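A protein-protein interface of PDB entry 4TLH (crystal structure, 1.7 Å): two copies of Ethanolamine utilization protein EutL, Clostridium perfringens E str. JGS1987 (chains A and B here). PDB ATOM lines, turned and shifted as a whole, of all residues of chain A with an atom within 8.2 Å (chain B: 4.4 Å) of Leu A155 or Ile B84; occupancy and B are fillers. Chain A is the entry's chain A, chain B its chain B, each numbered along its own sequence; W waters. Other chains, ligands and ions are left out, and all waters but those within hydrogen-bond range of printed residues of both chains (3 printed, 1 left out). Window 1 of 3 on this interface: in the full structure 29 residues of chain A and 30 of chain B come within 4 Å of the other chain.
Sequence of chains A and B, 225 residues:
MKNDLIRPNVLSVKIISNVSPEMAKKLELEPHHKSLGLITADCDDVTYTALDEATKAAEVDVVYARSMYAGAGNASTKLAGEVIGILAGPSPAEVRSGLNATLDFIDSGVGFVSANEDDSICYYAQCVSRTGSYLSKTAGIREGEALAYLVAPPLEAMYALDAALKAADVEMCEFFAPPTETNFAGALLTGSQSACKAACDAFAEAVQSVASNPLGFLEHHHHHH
The side-chain hydroxyl (OH) of Tyr B64 is in hydrogen-bond range of the backbone carbonyl oxygen (O) of Pro A178 (2.6 Å). The backbone carbonyl oxygen of Pro A214 is in hydrogen-bond range of the backbone NH of Val B13, at 3.0 Å. The backbone NH of Gly A216 lies within hydrogen-bond range of the backbone carbonyl oxygen of Val B13 (3.3 Å). O of Pro A214 lies within hydrogen-bond range of OG of Ser B12 (2.7 Å).
The backbone carbonyl oxygen of Ser B12 is in hydrogen-bond range of the backbone NH of Thr B40, 3.0 Å away. The backbone carbonyl oxygen (O) of Lys B14 lies within hydrogen-bond range of the backbone NH (N) of Leu B38 (2.7 Å). N of Gly B85 sits at hydrogen-bond distance from O of Ile B39, 2.9 Å away. ND2 of Asn A213 is in hydrogen-bond range of O of Gly A216 (3.1 Å). N of Ile B84 is in hydrogen-bond range of O of Arg B66, at 3.0 Å.
Leu A155 touches Ser B12. Ile B39 touches Leu A155. CE1 of Tyr A159 touches CE of Lys B14, 3.5 Å away. Tyr A159 touches Leu B38. Ala A177 touches Tyr B64 (CB to OH, 3.3 Å). O of Pro A178 touches CB of Arg B66 (3.6 Å). CD of Pro A179 touches NH2 of Arg B66 (3.7 Å). Met B68 touches Pro A179 (SD to CB, 3.8 Å). Leu A215 touches Ser B12 (CD2 to N, 3.8 Å). O of Val B13 touches C of Leu A215, at 3.6 Å.
Of chain B, only Ser B12 (3.5 Å), Leu B38 (3.5 Å), Ile B39 (3.8 Å), Thr B40 (3.7 Å) and Ile B84 (3.8 Å) come within 4 Å of Leu A155. Of chain A, only Pro A154 (3.7 Å), Leu A155 (3.8 Å) and Met A158 (3.96 Å) come within 4 Å of Ile B84. No residue of chain A comes within 4 Å of Val B83. Of the printed residues of chain A, Lys B14 touches Tyr A159. Of the printed residues of chain B, Pro A178 touches Tyr B64 and Arg B66. Printed residues of chain B within 4 Å of Tyr A159: Lys B14 (3.5 Å) and Leu B38 (3.8 Å). Printed residues of chain B within 4 Å of Met A158: Ile B84. Printed residues of chain A within 4 Å of Arg B66: Pro A178 (3.6 Å) and Pro A179 (3.7 Å). The nearest residue of chain B that does not touch Leu A155 is Lys B14 (4.1 Å). The nearest residue of chain A that does not touch Ile B84 is Pro A178 (4.3 Å).
Printed residues of chain B that touch a printed residue of chain A: Ser B12, Val B13, Lys B14, Leu B38, Ile B39, Thr B40, Tyr B64, Arg B66, Met B68 and Ile B84. Hydrophobic or aromatic side chains of chain B that line the printed part of chain A: Leu B38, Tyr B64, Met B68 and Ile B84. Along chain B the printed residues that touch a printed residue of chain A span positions 12 to 84. Among the printed residues, 21 pairs touch across the chains.
No position is printed for both chains. Of the 21 pairs that touch across the chains among the printed residues, none has its exchanged pair printed and touching as well.
Water W3 bridges NZ of Lys B14 (2.5 Å) and O of Asn A213 (3.0 Å). Water W1 lies within hydrogen-bond range of the guanidinium group (NH2) of Arg B66 and the backbone carbonyl oxygen (O) of Pro A179. Water W2 lies within hydrogen-bond range of the guanidinium group (NH1) of Arg B66, the backbone carbonyl oxygen (O) of Pro A179 and the backbone carbonyl oxygen (O) of Ala A177.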
ATOM      1  N   ALA A 152       6.929 -20.359   5.123  1.00  0.00           N
ATOM      2  CA  ALA A 152       8.160 -20.427   5.914  1.00  0.00           C
ATOM      3  C   ALA A 152       8.671 -21.865   5.873  1.00  0.00           C
ATOM      4  O   ALA A 152       7.966 -22.747   5.399  1.00  0.00           O
ATOM      5  CB  ALA A 152       7.922 -19.978   7.347  1.00  0.00           C
ATOM      6  N   PRO A 153       9.887 -22.125   6.383  1.00  0.00           N
ATOM      7  CA  PRO A 153      10.322 -23.522   6.422  1.00  0.00           C
ATOM      8  C   PRO A 153       9.408 -24.333   7.322  1.00  0.00           C
ATOM      9  O   PRO A 153       8.663 -23.723   8.102  1.00  0.00           O
ATOM     10  CB  PRO A 153      11.757 -23.439   6.960  1.00  0.00           C
ATOM     11  CG  PRO A 153      12.194 -22.049   6.660  1.00  0.00           C
ATOM     12  CD  PRO A 153      10.971 -21.201   6.756  1.00  0.00           C
ATOM     13  N   PRO A 154       9.450 -25.674   7.231  1.00  0.00           N
ATOM     14  CA  PRO A 154       8.372 -26.506   7.793  1.00  0.00           C
ATOM     15  C   PRO A 154       8.013 -26.290   9.284  1.00  0.00           C
ATOM     16  O   PRO A 154       6.837 -26.049   9.549  1.00  0.00           O
ATOM     17  CB  PRO A 154       8.893 -27.926   7.561  1.00  0.00           C
ATOM     18  CG  PRO A 154       9.705 -27.804   6.311  1.00  0.00           C
ATOM     19  CD  PRO A 154      10.398 -26.481   6.430  1.00  0.00           C
ATOM     20  N   LEU A 155       8.952 -26.345  10.214  1.00  0.00           N
ATOM     21  CA  LEU A 155       8.579 -26.199  11.620  1.00  0.00           C
ATOM     22  C   LEU A 155       8.091 -24.778  11.867  1.00  0.00           C
ATOM     23  O   LEU A 155       7.081 -24.573  12.540  1.00  0.00           O
ATOM     24  CB  LEU A 155       9.736 -26.514  12.573  1.00  0.00           C
ATOM     25  CG  LEU A 155       9.416 -26.494  14.068  1.00  0.00           C
ATOM     26  CD1 LEU A 155      10.183 -27.561  14.833  1.00  0.00           C
ATOM     27  CD2 LEU A 155       9.677 -25.111  14.689  1.00  0.00           C
ATOM     28  N   GLU A 156       8.810 -23.804  11.321  1.00  0.00           N
ATOM     29  CA  GLU A 156       8.475 -22.395  11.544  1.00  0.00           C
ATOM     30  C   GLU A 156       7.074 -22.099  11.019  1.00  0.00           C
ATOM     31  O   GLU A 156       6.288 -21.365  11.631  1.00  0.00           O
ATOM     32  CB  GLU A 156       9.492 -21.463  10.860  1.00  0.00           C
ATOM     33  CG  GLU A 156      10.932 -21.604  11.344  1.00  0.00           C
ATOM     34  CD  GLU A 156      11.740 -22.615  10.521  1.00  0.00           C
ATOM     35  OE1 GLU A 156      11.268 -23.758  10.335  1.00  0.00           O
ATOM     36  OE2 GLU A 156      12.852 -22.262  10.055  1.00  0.00           O
ATOM     37  N   ALA A 157       6.782 -22.660   9.848  1.00  0.00           N
ATOM     38  CA  ALA A 157       5.492 -22.473   9.208  1.00  0.00           C
ATOM     39  C   ALA A 157       4.341 -23.079   9.989  1.00  0.00           C
ATOM     40  O   ALA A 157       3.292 -22.449  10.131  1.00  0.00           O
ATOM     41  CB  ALA A 157       5.513 -23.069   7.811  1.00  0.00           C
ATOM     42  N   MET A 158       4.503 -24.315  10.448  1.00  0.00           N
ATOM     43  CA  MET A 158       3.443 -24.969  11.218  1.00  0.00           C
ATOM     44  C   MET A 158       3.176 -24.200  12.499  1.00  0.00           C
ATOM     45  O   MET A 158       2.025 -23.999  12.875  1.00  0.00           O
ATOM     46  CB  MET A 158       3.789 -26.432  11.557  1.00  0.00           C
ATOM     47  CG  MET A 158       3.967 -27.343  10.338  1.00  0.00           C
ATOM     48  SD  MET A 158       2.538 -27.267   9.253  1.00  0.00           S
ATOM     49  CE  MET A 158       1.371 -28.266  10.177  1.00  0.00           C
ATOM     50  N   TYR A 159       4.228 -23.764  13.173  1.00  0.00           N
ATOM     51  CA  TYR A 159       4.077 -22.951  14.375  1.00  0.00           C
ATOM     52  C   TYR A 159       3.410 -21.602  14.123  1.00  0.00           C
ATOM     53  O   TYR A 159       2.455 -21.230  14.792  1.00  0.00           O
ATOM     54  CB  TYR A 159       5.436 -22.713  15.028  1.00  0.00           C
ATOM     55  CG  TYR A 159       5.318 -21.950  16.325  1.00  0.00           C
ATOM     56  CD1 TYR A 159       4.875 -22.573  17.474  1.00  0.00           C
ATOM     57  CD2 TYR A 159       5.638 -20.604  16.393  1.00  0.00           C
ATOM     58  CE1 TYR A 159       4.762 -21.868  18.672  1.00  0.00           C
ATOM     59  CE2 TYR A 159       5.527 -19.903  17.555  1.00  0.00           C
ATOM     60  CZ  TYR A 159       5.082 -20.526  18.694  1.00  0.00           C
ATOM     61  OH  TYR A 159       4.991 -19.796  19.862  1.00  0.00           O
ATOM     62  N   ALA A 160       3.928 -20.876  13.149  1.00  0.00           N
ATOM     63  CA  ALA A 160       3.447 -19.537  12.841  1.00  0.00           C
ATOM     64  C   ALA A 160       2.061 -19.525  12.178  1.00  0.00           C
ATOM     65  O   ALA A 160       1.284 -18.577  12.340  1.00  0.00           O
ATOM     66  CB  ALA A 160       4.459 -18.836  11.977  1.00  0.00           C
ATOM     67  N   LEU A 161       1.731 -20.570  11.430  1.00  0.00           N
ATOM     68  CA  LEU A 161       0.394 -20.670  10.865  1.00  0.00           C
ATOM     69  C   LEU A 161      -0.628 -20.803  11.966  1.00  0.00           C
ATOM     70  O   LEU A 161      -1.646 -20.110  11.972  1.00  0.00           O
ATOM     71  CB  LEU A 161       0.267 -21.850   9.912  1.00  0.00           C
ATOM     72  CG  LEU A 161       0.852 -21.680   8.514  1.00  0.00           C
ATOM     73  CD1 LEU A 161       0.623 -22.945   7.738  1.00  0.00           C
ATOM     74  CD2 LEU A 161       0.255 -20.483   7.798  1.00  0.00           C
ATOM     75  N   ASP A 162      -0.358 -21.701  12.903  1.00  0.00           N
ATOM     76  CA  ASP A 162      -1.257 -21.889  14.000  1.00  0.00           C
ATOM     77  C   ASP A 162      -1.376 -20.585  14.779  1.00  0.00           C
ATOM     78  O   ASP A 162      -2.466 -20.206  15.205  1.00  0.00           O
ATOM     79  CB  ASP A 162      -0.785 -23.030  14.889  1.00  0.00           C
ATOM     80  CG  ASP A 162      -1.743 -23.302  16.003  1.00  0.00           C
ATOM     81  OD1 ASP A 162      -2.865 -23.777  15.729  1.00  0.00           O
ATOM     82  OD2 ASP A 162      -1.376 -23.014  17.142  1.00  0.00           O
ATOM     83  N   ALA A 177       1.210 -28.235   2.550  1.00  0.00           N
ATOM     84  CA  ALA A 177       1.733 -29.125   3.578  1.00  0.00           C
ATOM     85  C   ALA A 177       3.224 -29.346   3.370  1.00  0.00           C
ATOM     86  O   ALA A 177       3.666 -29.512   2.240  1.00  0.00           O
ATOM     87  CB  ALA A 177       0.982 -30.450   3.560  1.00  0.00           C
ATOM     88  N   PRO A 178       4.011 -29.339   4.460  1.00  0.00           N
ATOM     89  CA  PRO A 178       5.443 -29.563   4.276  1.00  0.00           C
ATOM     90  C   PRO A 178       5.750 -30.999   3.863  1.00  0.00           C
ATOM     91  O   PRO A 178       5.222 -31.952   4.425  1.00  0.00           O
ATOM     92  CB  PRO A 178       6.032 -29.234   5.652  1.00  0.00           C
ATOM     93  CG  PRO A 178       4.940 -29.423   6.591  1.00  0.00           C
ATOM     94  CD  PRO A 178       3.663 -29.136   5.874  1.00  0.00           C
ATOM     95  N   PRO A 179       6.626 -31.172   2.878  1.00  0.00           N
ATOM     96  CA  PRO A 179       7.353 -30.211   2.054  1.00  0.00           C
ATOM     97  C   PRO A 179       6.611 -29.796   0.789  1.00  0.00           C
ATOM     98  O   PRO A 179       6.030 -30.647   0.097  1.00  0.00           O
ATOM     99  CB  PRO A 179       8.607 -30.996   1.671  1.00  0.00           C
ATOM    100  CG  PRO A 179       8.101 -32.375   1.516  1.00  0.00           C
ATOM    101  CD  PRO A 179       7.060 -32.551   2.597  1.00  0.00           C
ATOM    102  N   ASN A 183      10.717 -27.302  -0.219  1.00  0.00           N
ATOM    103  CA  ASN A 183      10.902 -27.707   1.191  1.00  0.00           C
ATOM    104  C   ASN A 183      10.525 -26.597   2.161  1.00  0.00           C
ATOM    105  O   ASN A 183      11.146 -26.403   3.214  1.00  0.00           O
ATOM    106  CB  ASN A 183      12.331 -28.180   1.440  1.00  0.00           C
ATOM    107  CG  ASN A 183      12.625 -29.474   0.708  1.00  0.00           C
ATOM    108  OD1 ASN A 183      11.755 -30.338   0.600  1.00  0.00           O
ATOM    109  ND2 ASN A 183      13.827 -29.599   0.171  1.00  0.00           N
ATOM    110  N   PHE A 184       9.482 -25.884   1.764  1.00  0.00           N
ATOM    111  CA  PHE A 184       8.818 -24.899   2.590  1.00  0.00           C
ATOM    112  C   PHE A 184       7.419 -25.419   2.926  1.00  0.00           C
ATOM    113  O   PHE A 184       7.069 -26.571   2.623  1.00  0.00           O
ATOM    114  CB  PHE A 184       8.765 -23.547   1.862  1.00  0.00           C
ATOM    115  CG  PHE A 184      10.031 -22.750   1.981  1.00  0.00           C
ATOM    116  CD1 PHE A 184      11.164 -23.103   1.275  1.00  0.00           C
ATOM    117  CD2 PHE A 184      10.086 -21.655   2.797  1.00  0.00           C
ATOM    118  CE1 PHE A 184      12.328 -22.376   1.400  1.00  0.00           C
ATOM    119  CE2 PHE A 184      11.245 -20.918   2.923  1.00  0.00           C
ATOM    120  CZ  PHE A 184      12.363 -21.282   2.225  1.00  0.00           C
ATOM    121  N   ALA A 185       6.628 -24.577   3.582  1.00  0.00           N
ATOM    122  CA  ALA A 185       5.264 -24.908   3.979  1.00  0.00           C
ATOM    123  C   ALA A 185       4.525 -23.595   4.115  1.00  0.00           C
ATOM    124  O   ALA A 185       5.152 -22.532   4.192  1.00  0.00           O
ATOM    125  CB  ALA A 185       5.239 -25.673   5.287  1.00  0.00           C
ATOM    126  N   PHE A 203       2.026 -14.003  11.662  1.00  0.00           N
ATOM    127  CA  PHE A 203       2.848 -15.046  11.039  1.00  0.00           C
ATOM    128  C   PHE A 203       4.318 -14.676  11.117  1.00  0.00           C
ATOM    129  O   PHE A 203       5.149 -15.481  11.560  1.00  0.00           O
ATOM    130  CB  PHE A 203       2.429 -15.270   9.580  1.00  0.00           C
ATOM    131  CG  PHE A 203       3.129 -16.428   8.903  1.00  0.00           C
ATOM    132  CD1 PHE A 203       2.750 -17.727   9.166  1.00  0.00           C
ATOM    133  CD2 PHE A 203       4.154 -16.203   7.994  1.00  0.00           C
ATOM    134  CE1 PHE A 203       3.386 -18.804   8.526  1.00  0.00           C
ATOM    135  CE2 PHE A 203       4.790 -17.275   7.352  1.00  0.00           C
ATOM    136  CZ  PHE A 203       4.405 -18.559   7.631  1.00  0.00           C
ATOM    137  N   ALA A 206       5.855 -14.764  14.638  1.00  0.00           N
ATOM    138  CA  ALA A 206       5.963 -16.102  15.181  1.00  0.00           C
ATOM    139  C   ALA A 206       7.149 -16.818  14.548  1.00  0.00           C
ATOM    140  O   ALA A 206       7.862 -17.564  15.232  1.00  0.00           O
ATOM    141  CB  ALA A 206       4.691 -16.870  14.962  1.00  0.00           C
ATOM    142  N   VAL A 207       7.376 -16.587  13.253  1.00  0.00           N
ATOM    143  CA  VAL A 207       8.562 -17.157  12.601  1.00  0.00           C
ATOM    144  C   VAL A 207       9.836 -16.558  13.225  1.00  0.00           C
ATOM    145  O   VAL A 207      10.790 -17.280  13.519  1.00  0.00           O
ATOM    146  CB  VAL A 207       8.589 -16.918  11.081  1.00  0.00           C
ATOM    147  CG1 VAL A 207       9.886 -17.419  10.493  1.00  0.00           C
ATOM    148  CG2 VAL A 207       7.443 -17.628  10.396  1.00  0.00           C
ATOM    149  N   VAL A 210      10.625 -18.230  16.616  1.00  0.00           N
ATOM    150  CA  VAL A 210      11.271 -19.536  16.503  1.00  0.00           C
ATOM    151  C   VAL A 210      12.730 -19.361  16.078  1.00  0.00           C
ATOM    152  O   VAL A 210      13.648 -20.006  16.613  1.00  0.00           O
ATOM    153  CB  VAL A 210      10.547 -20.440  15.496  1.00  0.00           C
ATOM    154  CG1 VAL A 210      11.314 -21.739  15.285  1.00  0.00           C
ATOM    155  CG2 VAL A 210       9.145 -20.757  15.990  1.00  0.00           C
ATOM    156  N   ALA A 211      12.949 -18.462  15.129  1.00  0.00           N
ATOM    157  CA  ALA A 211      14.286 -18.282  14.596  1.00  0.00           C
ATOM    158  C   ALA A 211      15.236 -17.830  15.694  1.00  0.00           C
ATOM    159  O   ALA A 211      16.402 -18.206  15.705  1.00  0.00           O
ATOM    160  CB  ALA A 211      14.270 -17.294  13.451  1.00  0.00           C
ATOM    161  N   ASN A 213      15.176 -18.700  18.745  1.00  0.00           N
ATOM    162  CA  ASN A 213      15.405 -19.763  19.723  1.00  0.00           C
ATOM    163  C   ASN A 213      14.942 -21.104  19.172  1.00  0.00           C
ATOM    164  O   ASN A 213      13.904 -21.628  19.578  1.00  0.00           O
ATOM    165  CB  ASN A 213      14.690 -19.459  21.023  1.00  0.00           C
ATOM    166  CG  ASN A 213      15.040 -20.444  22.101  1.00  0.00           C
ATOM    167  OD1 ASN A 213      16.177 -20.918  22.176  1.00  0.00           O
ATOM    168  ND2 ASN A 213      14.066 -20.785  22.923  1.00  0.00           N
ATOM    169  N   PRO A 214      15.704 -21.645  18.219  1.00  0.00           N
ATOM    170  CA  PRO A 214      15.304 -22.820  17.437  1.00  0.00           C
ATOM    171  C   PRO A 214      15.040 -24.067  18.282  1.00  0.00           C
ATOM    172  O   PRO A 214      14.209 -24.879  17.891  1.00  0.00           O
ATOM    173  CB  PRO A 214      16.504 -23.050  16.511  1.00  0.00           C
ATOM    174  CG  PRO A 214      17.234 -21.776  16.474  1.00  0.00           C
ATOM    175  CD  PRO A 214      17.011 -21.115  17.794  1.00  0.00           C
ATOM    176  N   LEU A 215      15.716 -24.208  19.415  1.00  0.00           N
ATOM    177  CA  LEU A 215      15.563 -25.412  20.221  1.00  0.00           C
ATOM    178  C   LEU A 215      14.564 -25.247  21.380  1.00  0.00           C
ATOM    179  O   LEU A 215      14.523 -26.069  22.298  1.00  0.00           O
ATOM    180  CB  LEU A 215      16.929 -25.854  20.736  1.00  0.00           C
ATOM    181  CG  LEU A 215      17.807 -26.581  19.713  1.00  0.00           C
ATOM    182  CD1 LEU A 215      19.107 -26.942  20.386  1.00  0.00           C
ATOM    183  CD2 LEU A 215      17.116 -27.834  19.130  1.00  0.00           C
ATOM    184  N   GLY A 216      13.726 -24.217  21.296  1.00  0.00           N
ATOM    185  CA  GLY A 216      12.659 -24.007  22.261  1.00  0.00           C
ATOM    186  C   GLY A 216      13.082 -24.216  23.706  1.00  0.00           C
ATOM    187  O   GLY A 216      14.081 -23.651  24.164  1.00  0.00           O
ATOM    188  N   SER B  12      15.595 -28.371  15.655  1.00  0.00           N
ATOM    189  CA  SER B  12      14.593 -27.459  16.184  1.00  0.00           C
ATOM    190  C   SER B  12      13.497 -28.227  16.892  1.00  0.00           C
ATOM    191  O   SER B  12      13.109 -29.325  16.454  1.00  0.00           O
ATOM    192  CB  SER B  12      13.996 -26.617  15.046  1.00  0.00           C
ATOM    193  OG  SER B  12      13.061 -25.666  15.525  1.00  0.00           O
ATOM    194  N   VAL B  13      12.971 -27.604  17.936  1.00  0.00           N
ATOM    195  CA  VAL B  13      11.955 -28.166  18.815  1.00  0.00           C
ATOM    196  C   VAL B  13      11.003 -27.039  19.238  1.00  0.00           C
ATOM    197  O   VAL B  13      11.465 -25.966  19.626  1.00  0.00           O
ATOM    198  CB  VAL B  13      12.598 -28.796  20.078  1.00  0.00           C
ATOM    199  CG1 VAL B  13      11.548 -29.397  20.998  1.00  0.00           C
ATOM    200  CG2 VAL B  13      13.656 -29.825  19.700  1.00  0.00           C
ATOM    201  N   LYS B  14       9.689 -27.259  19.183  1.00  0.00           N
ATOM    202  CA  LYS B  14       8.755 -26.254  19.676  1.00  0.00           C
ATOM    203  C   LYS B  14       7.476 -26.905  20.163  1.00  0.00           C
ATOM    204  O   LYS B  14       7.015 -27.871  19.566  1.00  0.00           O
ATOM    205  CB  LYS B  14       8.446 -25.232  18.580  1.00  0.00           C
ATOM    206  CG  LYS B  14       7.648 -24.022  19.023  1.00  0.00           C
ATOM    207  CD  LYS B  14       8.538 -23.052  19.784  1.00  0.00           C
ATOM    208  CE  LYS B  14       7.762 -21.903  20.379  1.00  0.00           C
ATOM    209  NZ  LYS B  14       8.672 -20.968  21.076  1.00  0.00           N
ATOM    210  N   LEU B  38       6.556 -29.995  17.902  1.00  0.00           N
ATOM    211  CA  LEU B  38       7.165 -29.985  16.575  1.00  0.00           C
ATOM    212  C   LEU B  38       8.642 -30.297  16.711  1.00  0.00           C
ATOM    213  O   LEU B  38       9.293 -29.837  17.641  1.00  0.00           O
ATOM    214  CB  LEU B  38       6.987 -28.627  15.896  1.00  0.00           C
ATOM    215  CG  LEU B  38       5.591 -28.009  15.827  1.00  0.00           C
ATOM    216  CD1 LEU B  38       5.698 -26.559  15.295  1.00  0.00           C
ATOM    217  CD2 LEU B  38       4.644 -28.784  14.986  1.00  0.00           C
ATOM    218  N   ILE B  39       9.176 -31.081  15.784  1.00  0.00           N
ATOM    219  CA  ILE B  39      10.599 -31.376  15.777  1.00  0.00           C
ATOM    220  C   ILE B  39      11.124 -31.516  14.350  1.00  0.00           C
ATOM    221  O   ILE B  39      10.444 -32.067  13.483  1.00  0.00           O
ATOM    222  CB  ILE B  39      10.892 -32.659  16.596  1.00  0.00           C
ATOM    223  CG1 ILE B  39      12.399 -32.879  16.711  1.00  0.00           C
ATOM    224  CG2 ILE B  39      10.179 -33.868  15.974  1.00  0.00           C
ATOM    225  CD1 ILE B  39      12.800 -33.948  17.757  1.00  0.00           C
ATOM    226  N   THR B  40      12.318 -30.980  14.104  1.00  0.00           N
ATOM    227  CA  THR B  40      13.030 -31.269  12.859  1.00  0.00           C
ATOM    228  C   THR B  40      14.432 -31.779  13.140  1.00  0.00           C
ATOM    229  O   THR B  40      15.020 -31.511  14.201  1.00  0.00           O
ATOM    230  CB  THR B  40      13.129 -30.045  11.945  1.00  0.00           C
ATOM    231  OG1 THR B  40      13.923 -29.042  12.584  1.00  0.00           O
ATOM    232  CG2 THR B  40      11.737 -29.491  11.630  1.00  0.00           C
ATOM    233  N   TYR B  64       1.953 -36.124  12.265  1.00  0.00           N
ATOM    234  CA  TYR B  64       2.548 -35.621  11.029  1.00  0.00           C
ATOM    235  C   TYR B  64       3.971 -36.074  10.974  1.00  0.00           C
ATOM    236  O   TYR B  64       4.672 -36.041  11.967  1.00  0.00           O
ATOM    237  CB  TYR B  64       2.489 -34.094  10.932  1.00  0.00           C
ATOM    238  CG  TYR B  64       2.601 -33.590   9.504  1.00  0.00           C
ATOM    239  CD1 TYR B  64       3.839 -33.332   8.925  1.00  0.00           C
ATOM    240  CD2 TYR B  64       1.463 -33.365   8.743  1.00  0.00           C
ATOM    241  CE1 TYR B  64       3.943 -32.884   7.618  1.00  0.00           C
ATOM    242  CE2 TYR B  64       1.558 -32.914   7.425  1.00  0.00           C
ATOM    243  CZ  TYR B  64       2.805 -32.674   6.879  1.00  0.00           C
ATOM    244  OH  TYR B  64       2.910 -32.220   5.579  1.00  0.00           O
ATOM    245  N   ALA B  65       4.391 -36.561   9.811  1.00  0.00           N
ATOM    246  CA  ALA B  65       5.761 -36.987   9.650  1.00  0.00           C
ATOM    247  C   ALA B  65       6.086 -37.095   8.157  1.00  0.00           C
ATOM    248  O   ALA B  65       5.525 -37.921   7.459  1.00  0.00           O
ATOM    249  CB  ALA B  65       5.983 -38.315  10.366  1.00  0.00           C
ATOM    250  N   ARG B  66       6.996 -36.249   7.691  1.00  0.00           N
ATOM    251  CA  ARG B  66       7.345 -36.167   6.280  1.00  0.00           C
ATOM    252  C   ARG B  66       8.822 -35.808   6.111  1.00  0.00           C
ATOM    253  O   ARG B  66       9.410 -35.123   6.948  1.00  0.00           O
ATOM    254  CB  ARG B  66       6.469 -35.140   5.557  1.00  0.00           C
ATOM    255  CG  ARG B  66       4.986 -35.487   5.379  1.00  0.00           C
ATOM    256  CD  ARG B  66       4.734 -36.630   4.395  1.00  0.00           C
ATOM    257  NE  ARG B  66       5.426 -36.478   3.113  1.00  0.00           N
ATOM    258  CZ  ARG B  66       5.030 -35.677   2.119  1.00  0.00           C
ATOM    259  NH1 ARG B  66       3.944 -34.906   2.246  1.00  0.00           N
ATOM    260  NH2 ARG B  66       5.735 -35.627   0.995  1.00  0.00           N
ATOM    261  N   MET B  68      12.088 -34.343   3.572  1.00  0.00           N
ATOM    262  CA  MET B  68      12.342 -33.239   2.658  1.00  0.00           C
ATOM    263  C   MET B  68      13.038 -33.685   1.380  1.00  0.00           C
ATOM    264  O   MET B  68      13.906 -34.549   1.424  1.00  0.00           O
ATOM    265  CB  MET B  68      13.217 -32.188   3.331  1.00  0.00           C
ATOM    266  CG  MET B  68      12.680 -31.672   4.676  1.00  0.00           C
ATOM    267  SD  MET B  68      11.198 -30.669   4.474  1.00  0.00           S
ATOM    268  CE  MET B  68       9.991 -31.627   5.358  1.00  0.00           C
ATOM    269  N   VAL B  83      13.530 -33.771   7.828  1.00  0.00           N
ATOM    270  CA  VAL B  83      12.315 -34.352   8.377  1.00  0.00           C
ATOM    271  C   VAL B  83      11.624 -33.365   9.306  1.00  0.00           C
ATOM    272  O   VAL B  83      12.292 -32.604   9.990  1.00  0.00           O
ATOM    273  CB  VAL B  83      12.629 -35.678   9.125  1.00  0.00           C
ATOM    274  CG1 VAL B  83      13.510 -35.453  10.350  1.00  0.00           C
ATOM    275  CG2 VAL B  83      11.350 -36.410   9.500  1.00  0.00           C
ATOM    276  N   ILE B  84      10.292 -33.382   9.274  1.00  0.00           N
ATOM    277  CA  ILE B  84       9.479 -32.722  10.275  1.00  0.00           C
ATOM    278  C   ILE B  84       8.561 -33.781  10.843  1.00  0.00           C
ATOM    279  O   ILE B  84       7.957 -34.562  10.101  1.00  0.00           O
ATOM    280  CB  ILE B  84       8.664 -31.531   9.714  1.00  0.00           C
ATOM    281  CG1 ILE B  84       7.774 -30.957  10.832  1.00  0.00           C
ATOM    282  CG2 ILE B  84       7.853 -31.923   8.462  1.00  0.00           C
ATOM    283  CD1 ILE B  84       7.146 -29.689  10.542  1.00  0.00           C
ATOM    284  N   GLY B  85       8.486 -33.801  12.163  1.00  0.00           N
ATOM    285  CA  GLY B  85       7.551 -34.646  12.867  1.00  0.00           C
ATOM    286  C   GLY B  85       6.711 -33.828  13.816  1.00  0.00           C
ATOM    287  O   GLY B  85       7.180 -32.814  14.328  1.00  0.00           O
HETATM  288  O   HOH W   1       5.263 -33.495  -0.840  1.00  0.00           O
HETATM  289  O   HOH W   2       3.546 -32.427   0.756  1.00  0.00           O
HETATM  290  O   HOH W   3      10.949 -21.176  20.119  1.00  0.00           O
